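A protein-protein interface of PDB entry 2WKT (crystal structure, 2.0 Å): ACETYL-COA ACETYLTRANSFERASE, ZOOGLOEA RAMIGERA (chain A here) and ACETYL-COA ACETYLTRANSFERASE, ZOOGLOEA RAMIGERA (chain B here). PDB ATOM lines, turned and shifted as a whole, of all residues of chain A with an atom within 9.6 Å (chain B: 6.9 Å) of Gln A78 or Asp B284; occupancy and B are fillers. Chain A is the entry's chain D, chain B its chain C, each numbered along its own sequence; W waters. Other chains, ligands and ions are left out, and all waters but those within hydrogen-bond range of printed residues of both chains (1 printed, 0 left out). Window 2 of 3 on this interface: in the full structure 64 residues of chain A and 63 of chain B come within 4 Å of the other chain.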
ATOM      1  N   ALA A  46      -9.890 -19.268 -26.615  1.00  0.00           N
ATOM      2  CA  ALA A  46      -9.732 -19.816 -25.275  1.00  0.00           C
ATOM      3  C   ALA A  46      -9.759 -21.331 -25.333  1.00  0.00           C
ATOM      4  O   ALA A  46      -9.097 -22.008 -24.548  1.00  0.00           O
ATOM      5  CB  ALA A  46     -10.835 -19.296 -24.346  1.00  0.00           C
ATOM      6  N   GLY A  47     -10.520 -21.853 -26.286  1.00  0.00           N
ATOM      7  CA  GLY A  47     -10.640 -23.284 -26.480  1.00  0.00           C
ATOM      8  C   GLY A  47      -9.336 -23.927 -26.905  1.00  0.00           C
ATOM      9  O   GLY A  47      -9.212 -25.153 -26.891  1.00  0.00           O
ATOM     10  N   VAL A  49      -6.441 -23.121 -25.328  1.00  0.00           N
ATOM     11  CA  VAL A  49      -5.616 -23.235 -24.120  1.00  0.00           C
ATOM     12  C   VAL A  49      -5.617 -24.662 -23.556  1.00  0.00           C
ATOM     13  O   VAL A  49      -6.681 -25.209 -23.256  1.00  0.00           O
ATOM     14  CB  VAL A  49      -6.132 -22.307 -22.993  1.00  0.00           C
ATOM     15  CG1 VAL A  49      -5.285 -22.483 -21.712  1.00  0.00           C
ATOM     16  CG2 VAL A  49      -6.133 -20.844 -23.449  1.00  0.00           C
ATOM     17  N   ASN A  50      -4.441 -25.265 -23.398  1.00  0.00           N
ATOM     18  CA  ASN A  50      -4.364 -26.549 -22.701  1.00  0.00           C
ATOM     19  C   ASN A  50      -4.518 -26.421 -21.176  1.00  0.00           C
ATOM     20  O   ASN A  50      -5.221 -27.206 -20.548  1.00  0.00           O
ATOM     21  CB  ASN A  50      -3.058 -27.262 -23.018  1.00  0.00           C
ATOM     22  CG  ASN A  50      -2.903 -27.561 -24.499  1.00  0.00           C
ATOM     23  OD1 ASN A  50      -1.924 -27.182 -25.108  1.00  0.00           O
ATOM     24  ND2 ASN A  50      -3.896 -28.219 -25.083  1.00  0.00           N
ATOM     25  N   GLU A  51      -3.865 -25.425 -20.589  1.00  0.00           N
ATOM     26  CA  GLU A  51      -3.822 -25.309 -19.134  1.00  0.00           C
ATOM     27  C   GLU A  51      -3.519 -23.884 -18.705  1.00  0.00           C
ATOM     28  O   GLU A  51      -2.770 -23.188 -19.380  1.00  0.00           O
ATOM     29  CB  GLU A  51      -2.756 -26.257 -18.569  1.00  0.00           C
ATOM     30  CG  GLU A  51      -2.806 -26.437 -17.060  1.00  0.00           C
ATOM     31  CD  GLU A  51      -2.071 -27.693 -16.605  1.00  0.00           C
ATOM     32  OE1 GLU A  51      -0.835 -27.760 -16.799  1.00  0.00           O
ATOM     33  OE2 GLU A  51      -2.733 -28.608 -16.061  1.00  0.00           O
ATOM     34  N   ARG A  68      -8.586 -22.382 -11.574  1.00  0.00           N
ATOM     35  CA  ARG A  68      -9.701 -22.934 -12.345  1.00  0.00           C
ATOM     36  C   ARG A  68     -10.838 -21.916 -12.457  1.00  0.00           C
ATOM     37  O   ARG A  68     -11.371 -21.703 -13.545  1.00  0.00           O
ATOM     38  CB  ARG A  68     -10.187 -24.231 -11.694  1.00  0.00           C
ATOM     39  CG  ARG A  68     -11.412 -24.908 -12.365  1.00  0.00           C
ATOM     40  CD  ARG A  68     -11.060 -25.500 -13.734  1.00  0.00           C
ATOM     41  NE  ARG A  68     -12.050 -26.478 -14.195  1.00  0.00           N
ATOM     42  CZ  ARG A  68     -12.006 -27.080 -15.387  1.00  0.00           C
ATOM     43  NH1 ARG A  68     -11.020 -26.801 -16.229  1.00  0.00           N
ATOM     44  NH2 ARG A  68     -12.943 -27.961 -15.738  1.00  0.00           N
ATOM     45  N   ALA A  71      -9.856 -19.308 -14.870  1.00  0.00           N
ATOM     46  CA  ALA A  71      -9.795 -19.850 -16.218  1.00  0.00           C
ATOM     47  C   ALA A  71     -11.191 -19.982 -16.826  1.00  0.00           C
ATOM     48  O   ALA A  71     -11.415 -19.632 -17.991  1.00  0.00           O
ATOM     49  CB  ALA A  71      -9.073 -21.194 -16.218  1.00  0.00           C
ATOM     50  N   MET A  72     -12.130 -20.468 -16.026  1.00  0.00           N
ATOM     51  CA  MET A  72     -13.483 -20.705 -16.495  1.00  0.00           C
ATOM     52  C   MET A  72     -14.252 -19.410 -16.732  1.00  0.00           C
ATOM     53  O   MET A  72     -15.081 -19.327 -17.633  1.00  0.00           O
ATOM     54  CB  MET A  72     -14.230 -21.604 -15.524  1.00  0.00           C
ATOM     55  CG  MET A  72     -13.663 -23.009 -15.466  1.00  0.00           C
ATOM     56  SD  MET A  72     -14.532 -24.109 -16.590  1.00  0.00           S
ATOM     57  CE  MET A  72     -16.079 -24.316 -15.716  1.00  0.00           C
ATOM     58  N   LYS A  73     -13.970 -18.390 -15.937  1.00  0.00           N
ATOM     59  CA  LYS A  73     -14.649 -17.118 -16.126  1.00  0.00           C
ATOM     60  C   LYS A  73     -14.129 -16.439 -17.386  1.00  0.00           C
ATOM     61  O   LYS A  73     -14.832 -15.651 -18.015  1.00  0.00           O
ATOM     62  CB  LYS A  73     -14.464 -16.210 -14.912  1.00  0.00           C
ATOM     63  CG  LYS A  73     -15.154 -14.873 -15.055  1.00  0.00           C
ATOM     64  CD  LYS A  73     -14.685 -13.912 -13.981  1.00  0.00           C
ATOM     65  CE  LYS A  73     -15.488 -12.621 -14.004  1.00  0.00           C
ATOM     66  NZ  LYS A  73     -16.936 -12.881 -13.799  1.00  0.00           N
ATOM     67  N   GLY A  75     -13.430 -17.887 -20.085  1.00  0.00           N
ATOM     68  CA  GLY A  75     -13.958 -18.560 -21.256  1.00  0.00           C
ATOM     69  C   GLY A  75     -13.259 -19.867 -21.586  1.00  0.00           C
ATOM     70  O   GLY A  75     -13.732 -20.634 -22.421  1.00  0.00           O
ATOM     71  N   VAL A  76     -12.134 -20.134 -20.934  1.00  0.00           N
ATOM     72  CA  VAL A  76     -11.435 -21.389 -21.176  1.00  0.00           C
ATOM     73  C   VAL A  76     -12.364 -22.571 -20.850  1.00  0.00           C
ATOM     74  O   VAL A  76     -12.831 -22.710 -19.721  1.00  0.00           O
ATOM     75  CB  VAL A  76     -10.126 -21.458 -20.378  1.00  0.00           C
ATOM     76  CG1 VAL A  76      -9.333 -22.683 -20.784  1.00  0.00           C
ATOM     77  CG2 VAL A  76      -9.311 -20.198 -20.616  1.00  0.00           C
ATOM     78  N   PRO A  77     -12.644 -23.422 -21.847  1.00  0.00           N
ATOM     79  CA  PRO A  77     -13.628 -24.512 -21.707  1.00  0.00           C
ATOM     80  C   PRO A  77     -13.289 -25.474 -20.569  1.00  0.00           C
ATOM     81  O   PRO A  77     -12.203 -25.375 -20.005  1.00  0.00           O
ATOM     82  CB  PRO A  77     -13.555 -25.239 -23.060  1.00  0.00           C
ATOM     83  CG  PRO A  77     -12.255 -24.825 -23.666  1.00  0.00           C
ATOM     84  CD  PRO A  77     -11.938 -23.456 -23.140  1.00  0.00           C
ATOM     85  N   GLN A  78     -14.198 -26.394 -20.255  1.00  0.00           N
ATOM     86  CA  GLN A  78     -14.040 -27.288 -19.103  1.00  0.00           C
ATOM     87  C   GLN A  78     -12.947 -28.328 -19.359  1.00  0.00           C
ATOM     88  O   GLN A  78     -12.269 -28.784 -18.435  1.00  0.00           O
ATOM     89  CB  GLN A  78     -15.374 -27.975 -18.769  1.00  0.00           C
ATOM     90  CG  GLN A  78     -15.963 -28.758 -19.940  1.00  0.00           C
ATOM     91  CD  GLN A  78     -17.398 -29.227 -19.716  1.00  0.00           C
ATOM     92  OE1 GLN A  78     -17.823 -30.246 -20.280  1.00  0.00           O
ATOM     93  NE2 GLN A  78     -18.157 -28.482 -18.900  1.00  0.00           N
ATOM     94  N   GLU A  79     -12.776 -28.687 -20.628  1.00  0.00           N
ATOM     95  CA  GLU A  79     -11.781 -29.666 -21.026  1.00  0.00           C
ATOM     96  C   GLU A  79     -10.356 -29.293 -20.606  1.00  0.00           C
ATOM     97  O   GLU A  79      -9.557 -30.166 -20.316  1.00  0.00           O
ATOM     98  CB  GLU A  79     -11.849 -29.911 -22.549  1.00  0.00           C
ATOM     99  CG  GLU A  79     -10.992 -31.053 -23.016  1.00  0.00           C
ATOM    100  CD  GLU A  79     -10.963 -31.210 -24.529  1.00  0.00           C
ATOM    101  OE1 GLU A  79     -11.732 -30.516 -25.237  1.00  0.00           O
ATOM    102  OE2 GLU A  79     -10.166 -32.044 -25.003  1.00  0.00           O
ATOM    103  N   ALA A  80     -10.023 -28.009 -20.593  1.00  0.00           N
ATOM    104  CA  ALA A  80      -8.687 -27.599 -20.186  1.00  0.00           C
ATOM    105  C   ALA A  80      -8.454 -27.858 -18.683  1.00  0.00           C
ATOM    106  O   ALA A  80      -9.372 -28.222 -17.955  1.00  0.00           O
ATOM    107  CB  ALA A  80      -8.440 -26.128 -20.544  1.00  0.00           C
ATOM    108  N   THR A  81      -7.221 -27.694 -18.217  1.00  0.00           N
ATOM    109  CA  THR A  81      -6.956 -27.890 -16.796  1.00  0.00           C
ATOM    110  C   THR A  81      -6.456 -26.605 -16.181  1.00  0.00           C
ATOM    111  O   THR A  81      -6.045 -25.680 -16.897  1.00  0.00           O
ATOM    112  CB  THR A  81      -5.954 -29.040 -16.527  1.00  0.00           C
ATOM    113  OG1 THR A  81      -4.786 -28.863 -17.333  1.00  0.00           O
ATOM    114  CG2 THR A  81      -6.583 -30.381 -16.853  1.00  0.00           C
ATOM    115  N   ALA A  82      -6.523 -26.525 -14.856  1.00  0.00           N
ATOM    116  CA  ALA A  82      -5.971 -25.371 -14.174  1.00  0.00           C
ATOM    117  C   ALA A  82      -5.467 -25.746 -12.786  1.00  0.00           C
ATOM    118  O   ALA A  82      -5.984 -26.680 -12.157  1.00  0.00           O
ATOM    119  CB  ALA A  82      -7.004 -24.232 -14.118  1.00  0.00           C
ATOM    120  N   ASP B 150     -17.875 -26.920  -4.801  1.00  0.00           N
ATOM    121  CA  ASP B 150     -17.683 -26.471  -6.176  1.00  0.00           C
ATOM    122  C   ASP B 150     -17.933 -24.978  -6.320  1.00  0.00           C
ATOM    123  O   ASP B 150     -19.024 -24.489  -6.033  1.00  0.00           O
ATOM    124  CB  ASP B 150     -18.565 -27.234  -7.148  1.00  0.00           C
ATOM    125  CG  ASP B 150     -18.256 -26.890  -8.587  1.00  0.00           C
ATOM    126  OD1 ASP B 150     -17.289 -27.466  -9.146  1.00  0.00           O
ATOM    127  OD2 ASP B 150     -18.972 -26.038  -9.153  1.00  0.00           O
ATOM    128  N   TYR B 153     -20.953 -24.198  -8.854  1.00  0.00           N
ATOM    129  CA  TYR B 153     -22.311 -24.660  -8.554  1.00  0.00           C
ATOM    130  C   TYR B 153     -22.696 -24.509  -7.084  1.00  0.00           C
ATOM    131  O   TYR B 153     -23.877 -24.565  -6.739  1.00  0.00           O
ATOM    132  CB  TYR B 153     -22.522 -26.098  -9.041  1.00  0.00           C
ATOM    133  CG  TYR B 153     -22.548 -26.205 -10.550  1.00  0.00           C
ATOM    134  CD1 TYR B 153     -21.381 -26.417 -11.271  1.00  0.00           C
ATOM    135  CD2 TYR B 153     -23.738 -26.070 -11.255  1.00  0.00           C
ATOM    136  CE1 TYR B 153     -21.399 -26.504 -12.649  1.00  0.00           C
ATOM    137  CE2 TYR B 153     -23.768 -26.155 -12.635  1.00  0.00           C
ATOM    138  CZ  TYR B 153     -22.595 -26.371 -13.328  1.00  0.00           C
ATOM    139  OH  TYR B 153     -22.613 -26.462 -14.705  1.00  0.00           O
ATOM    140  N   THR B 160     -21.829 -33.530  -6.636  1.00  0.00           N
ATOM    141  CA  THR B 160     -21.277 -33.992  -7.921  1.00  0.00           C
ATOM    142  C   THR B 160     -21.345 -35.519  -7.954  1.00  0.00           C
ATOM    143  O   THR B 160     -21.625 -36.119  -8.992  1.00  0.00           O
ATOM    144  CB  THR B 160     -19.796 -33.556  -8.155  1.00  0.00           C
ATOM    145  OG1 THR B 160     -18.900 -34.458  -7.488  1.00  0.00           O
ATOM    146  CG2 THR B 160     -19.549 -32.131  -7.682  1.00  0.00           C
ATOM    147  N   VAL B 281      -6.710 -33.924 -17.618  1.00  0.00           N
ATOM    148  CA  VAL B 281      -7.771 -33.477 -18.506  1.00  0.00           C
ATOM    149  C   VAL B 281      -8.937 -32.872 -17.708  1.00  0.00           C
ATOM    150  O   VAL B 281      -9.161 -33.210 -16.533  1.00  0.00           O
ATOM    151  CB  VAL B 281      -8.279 -34.634 -19.433  1.00  0.00           C
ATOM    152  CG1 VAL B 281      -9.066 -34.080 -20.582  1.00  0.00           C
ATOM    153  CG2 VAL B 281      -7.113 -35.479 -19.965  1.00  0.00           C
ATOM    154  N   GLY B 282      -9.671 -31.964 -18.346  1.00  0.00           N
ATOM    155  CA  GLY B 282     -10.857 -31.369 -17.738  1.00  0.00           C
ATOM    156  C   GLY B 282     -12.158 -32.061 -18.116  1.00  0.00           C
ATOM    157  O   GLY B 282     -12.243 -32.740 -19.133  1.00  0.00           O
ATOM    158  N   VAL B 283     -13.174 -31.893 -17.276  1.00  0.00           N
ATOM    159  CA  VAL B 283     -14.512 -32.404 -17.537  1.00  0.00           C
ATOM    160  C   VAL B 283     -15.477 -31.435 -16.877  1.00  0.00           C
ATOM    161  O   VAL B 283     -15.059 -30.534 -16.145  1.00  0.00           O
ATOM    162  CB  VAL B 283     -14.735 -33.808 -16.910  1.00  0.00           C
ATOM    163  CG1 VAL B 283     -13.919 -34.886 -17.633  1.00  0.00           C
ATOM    164  CG2 VAL B 283     -14.403 -33.796 -15.423  1.00  0.00           C
ATOM    165  N   ASP B 284     -16.768 -31.623 -17.112  1.00  0.00           N
ATOM    166  CA  ASP B 284     -17.786 -30.791 -16.459  1.00  0.00           C
ATOM    167  C   ASP B 284     -17.639 -30.876 -14.938  1.00  0.00           C
ATOM    168  O   ASP B 284     -17.586 -31.967 -14.375  1.00  0.00           O
ATOM    169  CB  ASP B 284     -19.182 -31.238 -16.899  1.00  0.00           C
ATOM    170  CG  ASP B 284     -20.277 -30.287 -16.454  1.00  0.00           C
ATOM    171  OD1 ASP B 284     -20.085 -29.538 -15.479  1.00  0.00           O
ATOM    172  OD2 ASP B 284     -21.346 -30.298 -17.090  1.00  0.00           O
ATOM    173  N   PRO B 285     -17.561 -29.721 -14.263  1.00  0.00           N
ATOM    174  CA  PRO B 285     -17.471 -29.753 -12.799  1.00  0.00           C
ATOM    175  C   PRO B 285     -18.611 -30.542 -12.148  1.00  0.00           C
ATOM    176  O   PRO B 285     -18.401 -31.200 -11.126  1.00  0.00           O
ATOM    177  CB  PRO B 285     -17.546 -28.280 -12.411  1.00  0.00           C
ATOM    178  CG  PRO B 285     -17.127 -27.526 -13.628  1.00  0.00           C
ATOM    179  CD  PRO B 285     -17.578 -28.344 -14.794  1.00  0.00           C
ATOM    180  N   LYS B 286     -19.795 -30.493 -12.749  1.00  0.00           N
ATOM    181  CA  LYS B 286     -20.972 -31.160 -12.194  1.00  0.00           C
ATOM    182  C   LYS B 286     -20.769 -32.665 -11.992  1.00  0.00           C
ATOM    183  O   LYS B 286     -21.322 -33.248 -11.065  1.00  0.00           O
ATOM    184  CB  LYS B 286     -22.188 -30.926 -13.096  1.00  0.00           C
ATOM    185  CG  LYS B 286     -22.589 -29.475 -13.229  1.00  0.00           C
ATOM    186  CD  LYS B 286     -24.041 -29.341 -13.663  1.00  0.00           C
ATOM    187  CE  LYS B 286     -24.279 -29.983 -15.020  1.00  0.00           C
ATOM    188  NZ  LYS B 286     -23.656 -29.189 -16.113  1.00  0.00           N
ATOM    189  N   VAL B 287     -20.012 -33.291 -12.889  1.00  0.00           N
ATOM    190  CA  VAL B 287     -19.688 -34.708 -12.760  1.00  0.00           C
ATOM    191  C   VAL B 287     -18.168 -34.910 -12.728  1.00  0.00           C
ATOM    192  O   VAL B 287     -17.609 -35.724 -13.488  1.00  0.00           O
ATOM    193  CB  VAL B 287     -20.294 -35.521 -13.914  1.00  0.00           C
ATOM    194  CG1 VAL B 287     -21.800 -35.761 -13.669  1.00  0.00           C
ATOM    195  CG2 VAL B 287     -20.042 -34.803 -15.236  1.00  0.00           C
ATOM    196  N   MET B 288     -17.520 -34.134 -11.862  1.00  0.00           N
ATOM    197  CA  MET B 288     -16.067 -34.119 -11.715  1.00  0.00           C
ATOM    198  C   MET B 288     -15.485 -35.511 -11.517  1.00  0.00           C
ATOM    199  O   MET B 288     -14.323 -35.762 -11.833  1.00  0.00           O
ATOM    200  CB  MET B 288     -15.678 -33.228 -10.531  1.00  0.00           C
ATOM    201  CG  MET B 288     -16.062 -33.790  -9.169  1.00  0.00           C
ATOM    202  SD  MET B 288     -14.791 -34.811  -8.372  1.00  0.00           S
ATOM    203  CE  MET B 288     -15.617 -35.093  -6.800  1.00  0.00           C
ATOM    204  N   GLY B 289     -16.302 -36.412 -10.988  1.00  0.00           N
ATOM    205  CA  GLY B 289     -15.858 -37.756 -10.680  1.00  0.00           C
ATOM    206  C   GLY B 289     -15.545 -38.593 -11.906  1.00  0.00           C
ATOM    207  O   GLY B 289     -14.961 -39.673 -11.787  1.00  0.00           O
ATOM    208  N   THR B 290     -15.928 -38.099 -13.081  1.00  0.00           N
ATOM    209  CA  THR B 290     -15.614 -38.791 -14.337  1.00  0.00           C
ATOM    210  C   THR B 290     -14.197 -38.492 -14.831  1.00  0.00           C
ATOM    211  O   THR B 290     -13.695 -39.151 -15.755  1.00  0.00           O
ATOM    212  CB  THR B 290     -16.571 -38.390 -15.472  1.00  0.00           C
ATOM    213  OG1 THR B 290     -16.543 -36.970 -15.642  1.00  0.00           O
ATOM    214  CG2 THR B 290     -17.992 -38.852 -15.186  1.00  0.00           C
ATOM    215  N   GLY B 291     -13.575 -37.475 -14.236  1.00  0.00           N
ATOM    216  CA  GLY B 291     -12.241 -37.046 -14.615  1.00  0.00           C
ATOM    217  C   GLY B 291     -11.241 -38.164 -14.890  1.00  0.00           C
ATOM    218  O   GLY B 291     -10.498 -38.084 -15.863  1.00  0.00           O
ATOM    219  N   ILE B 379     -10.855 -34.831  -9.575  1.00  0.00           N
ATOM    220  CA  ILE B 379     -10.437 -33.523  -9.110  1.00  0.00           C
ATOM    221  C   ILE B 379     -11.651 -32.591  -9.095  1.00  0.00           C
ATOM    222  O   ILE B 379     -12.357 -32.478 -10.081  1.00  0.00           O
ATOM    223  CB  ILE B 379      -9.307 -32.974 -10.026  1.00  0.00           C
ATOM    224  CG1 ILE B 379      -8.111 -33.936 -10.007  1.00  0.00           C
ATOM    225  CG2 ILE B 379      -8.872 -31.585  -9.602  1.00  0.00           C
ATOM    226  CD1 ILE B 379      -6.995 -33.541 -10.928  1.00  0.00           C
ATOM    227  N   GLY B 381     -13.936 -29.332  -9.385  1.00  0.00           N
ATOM    228  CA  GLY B 381     -13.841 -28.325 -10.419  1.00  0.00           C
ATOM    229  C   GLY B 381     -13.848 -29.019 -11.771  1.00  0.00           C
ATOM    230  O   GLY B 381     -13.842 -28.366 -12.812  1.00  0.00           O
ATOM    231  N   GLY B 382     -13.871 -30.347 -11.749  1.00  0.00           N
ATOM    232  CA  GLY B 382     -13.980 -31.125 -12.970  1.00  0.00           C
ATOM    233  C   GLY B 382     -12.666 -31.295 -13.716  1.00  0.00           C
ATOM    234  O   GLY B 382     -12.474 -30.736 -14.791  1.00  0.00           O
ATOM    235  N   MET B 383     -11.752 -32.064 -13.134  1.00  0.00           N
ATOM    236  CA  MET B 383     -10.550 -32.487 -13.841  1.00  0.00           C
ATOM    237  C   MET B 383     -10.225 -33.909 -13.445  1.00  0.00           C
ATOM    238  O   MET B 383     -10.867 -34.472 -12.567  1.00  0.00           O
ATOM    239  CB  MET B 383      -9.349 -31.604 -13.500  1.00  0.00           C
ATOM    240  CG  MET B 383      -9.413 -30.190 -14.038  1.00  0.00           C
ATOM    241  SD  MET B 383      -8.046 -29.224 -13.364  1.00  0.00           S
ATOM    242  CE  MET B 383      -8.780 -28.677 -11.808  1.00  0.00           C
HETATM  243  O   HOH W   1     -17.954 -33.533 -19.097  1.00  0.00           O
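O of Gly B381 sits at hydrogen-bond distance from NE of Arg A68.
NH2 of Arg A68 is in hydrogen-bond range of O of Gly B382.
The backbone NH (N) of Gly B282 is in hydrogen-bond range of the backbone carbonyl oxygen (O) of Glu A79, 2.7 Å away.
NH2 of Arg A68 is in hydrogen-bond range of O of Val B283.
The side-chain sulfur of Met B383 sits at hydrogen-bond distance from the backbone NH of Ala A82.
The backbone NH (N) of Val B283 lies within hydrogen-bond range of the backbone carbonyl oxygen (O) of Gln A78 (3.4 Å).
The side-chain amino group of Lys B286 is in salt-bridge range of the side-chain carboxylate of Asp B284 (2.7 Å).
The guanidinium group (NH2) of Arg A68 is in hydrogen-bond range of the backbone carbonyl oxygen (O) of Gln A78, 2.9 Å away.
The side-chain hydroxyl (OG1) of Thr A81 is in hydrogen-bond range of the side-chain carboxylate (OE2) of Glu A51 (2.4 Å).
The backbone NH (N) of Val B283 lies within hydrogen-bond range of the backbone carbonyl oxygen (O) of Gly B382 (2.8 Å).
The backbone carbonyl oxygen (O) of Ala A80 is in hydrogen-bond range of the guanidinium group (NH1) of Arg A68 (2.8 Å).
The backbone NH (N) of Thr A81 sits at hydrogen-bond distance from the backbone carbonyl oxygen (O) of Asn A50.
Among the printed residues, pairs that only touch across the chains: Met A72 with Pro B285, Gln A78 with Gly B282, Gln A78 with Asp B284, Glu A79 with Val B281, Ala A80 with Gly B282, Thr A81 with Val B281, Thr A81 with Gly B282 and Thr A81 with Met B383.
Of chain B, only Gly B282 (3.0 Å), Val B283 (3.4 Å) and Asp B284 (3.4 Å) come within 4 Å of Gln A78.
Of the printed residues of chain B, Glu A79 touches Val B281 and Gly B282.
Printed residues of chain B within 4 Å of Ala A80: Gly B282.
Of the printed residues of chain B, Thr A81 touches Val B281, Gly B282 and Met B383.
Printed residues of chain B within 4 Å of Ala A82: Met B383 (3.4 Å).
Gly B282 touches just these residues of chain A: Gln A78, Glu A79, Ala A80 and Thr A81.
Val B283 touches just these residues of chain A: Arg A68 and Gln A78.
Of chain A, only Gln A78 (3.4 Å) comes within 4 Å of Asp B284.
Pro B285 touches just one residue of chain A: Met A72 (3.97 Å).
No residue of chain A comes within 4 Å of Lys B286.
Gly B382 touches just one residue of chain A: Arg A68 (3.0 Å).
The nearest printed residue of chain B that does not touch Gln A78 is Gly B382 (4.1 Å).
The nearest printed residue of chain B that does not touch Met A72 is Gly B381 (5.5 Å).
Hydrophobic or aromatic side chains of chain B that line the printed part of chain A: Val B281, Pro B285 and Met B383.
Water W1 bridges N of Asp B284 (3.0 Å) and OE1 of Gln A78 (3.5 Å).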
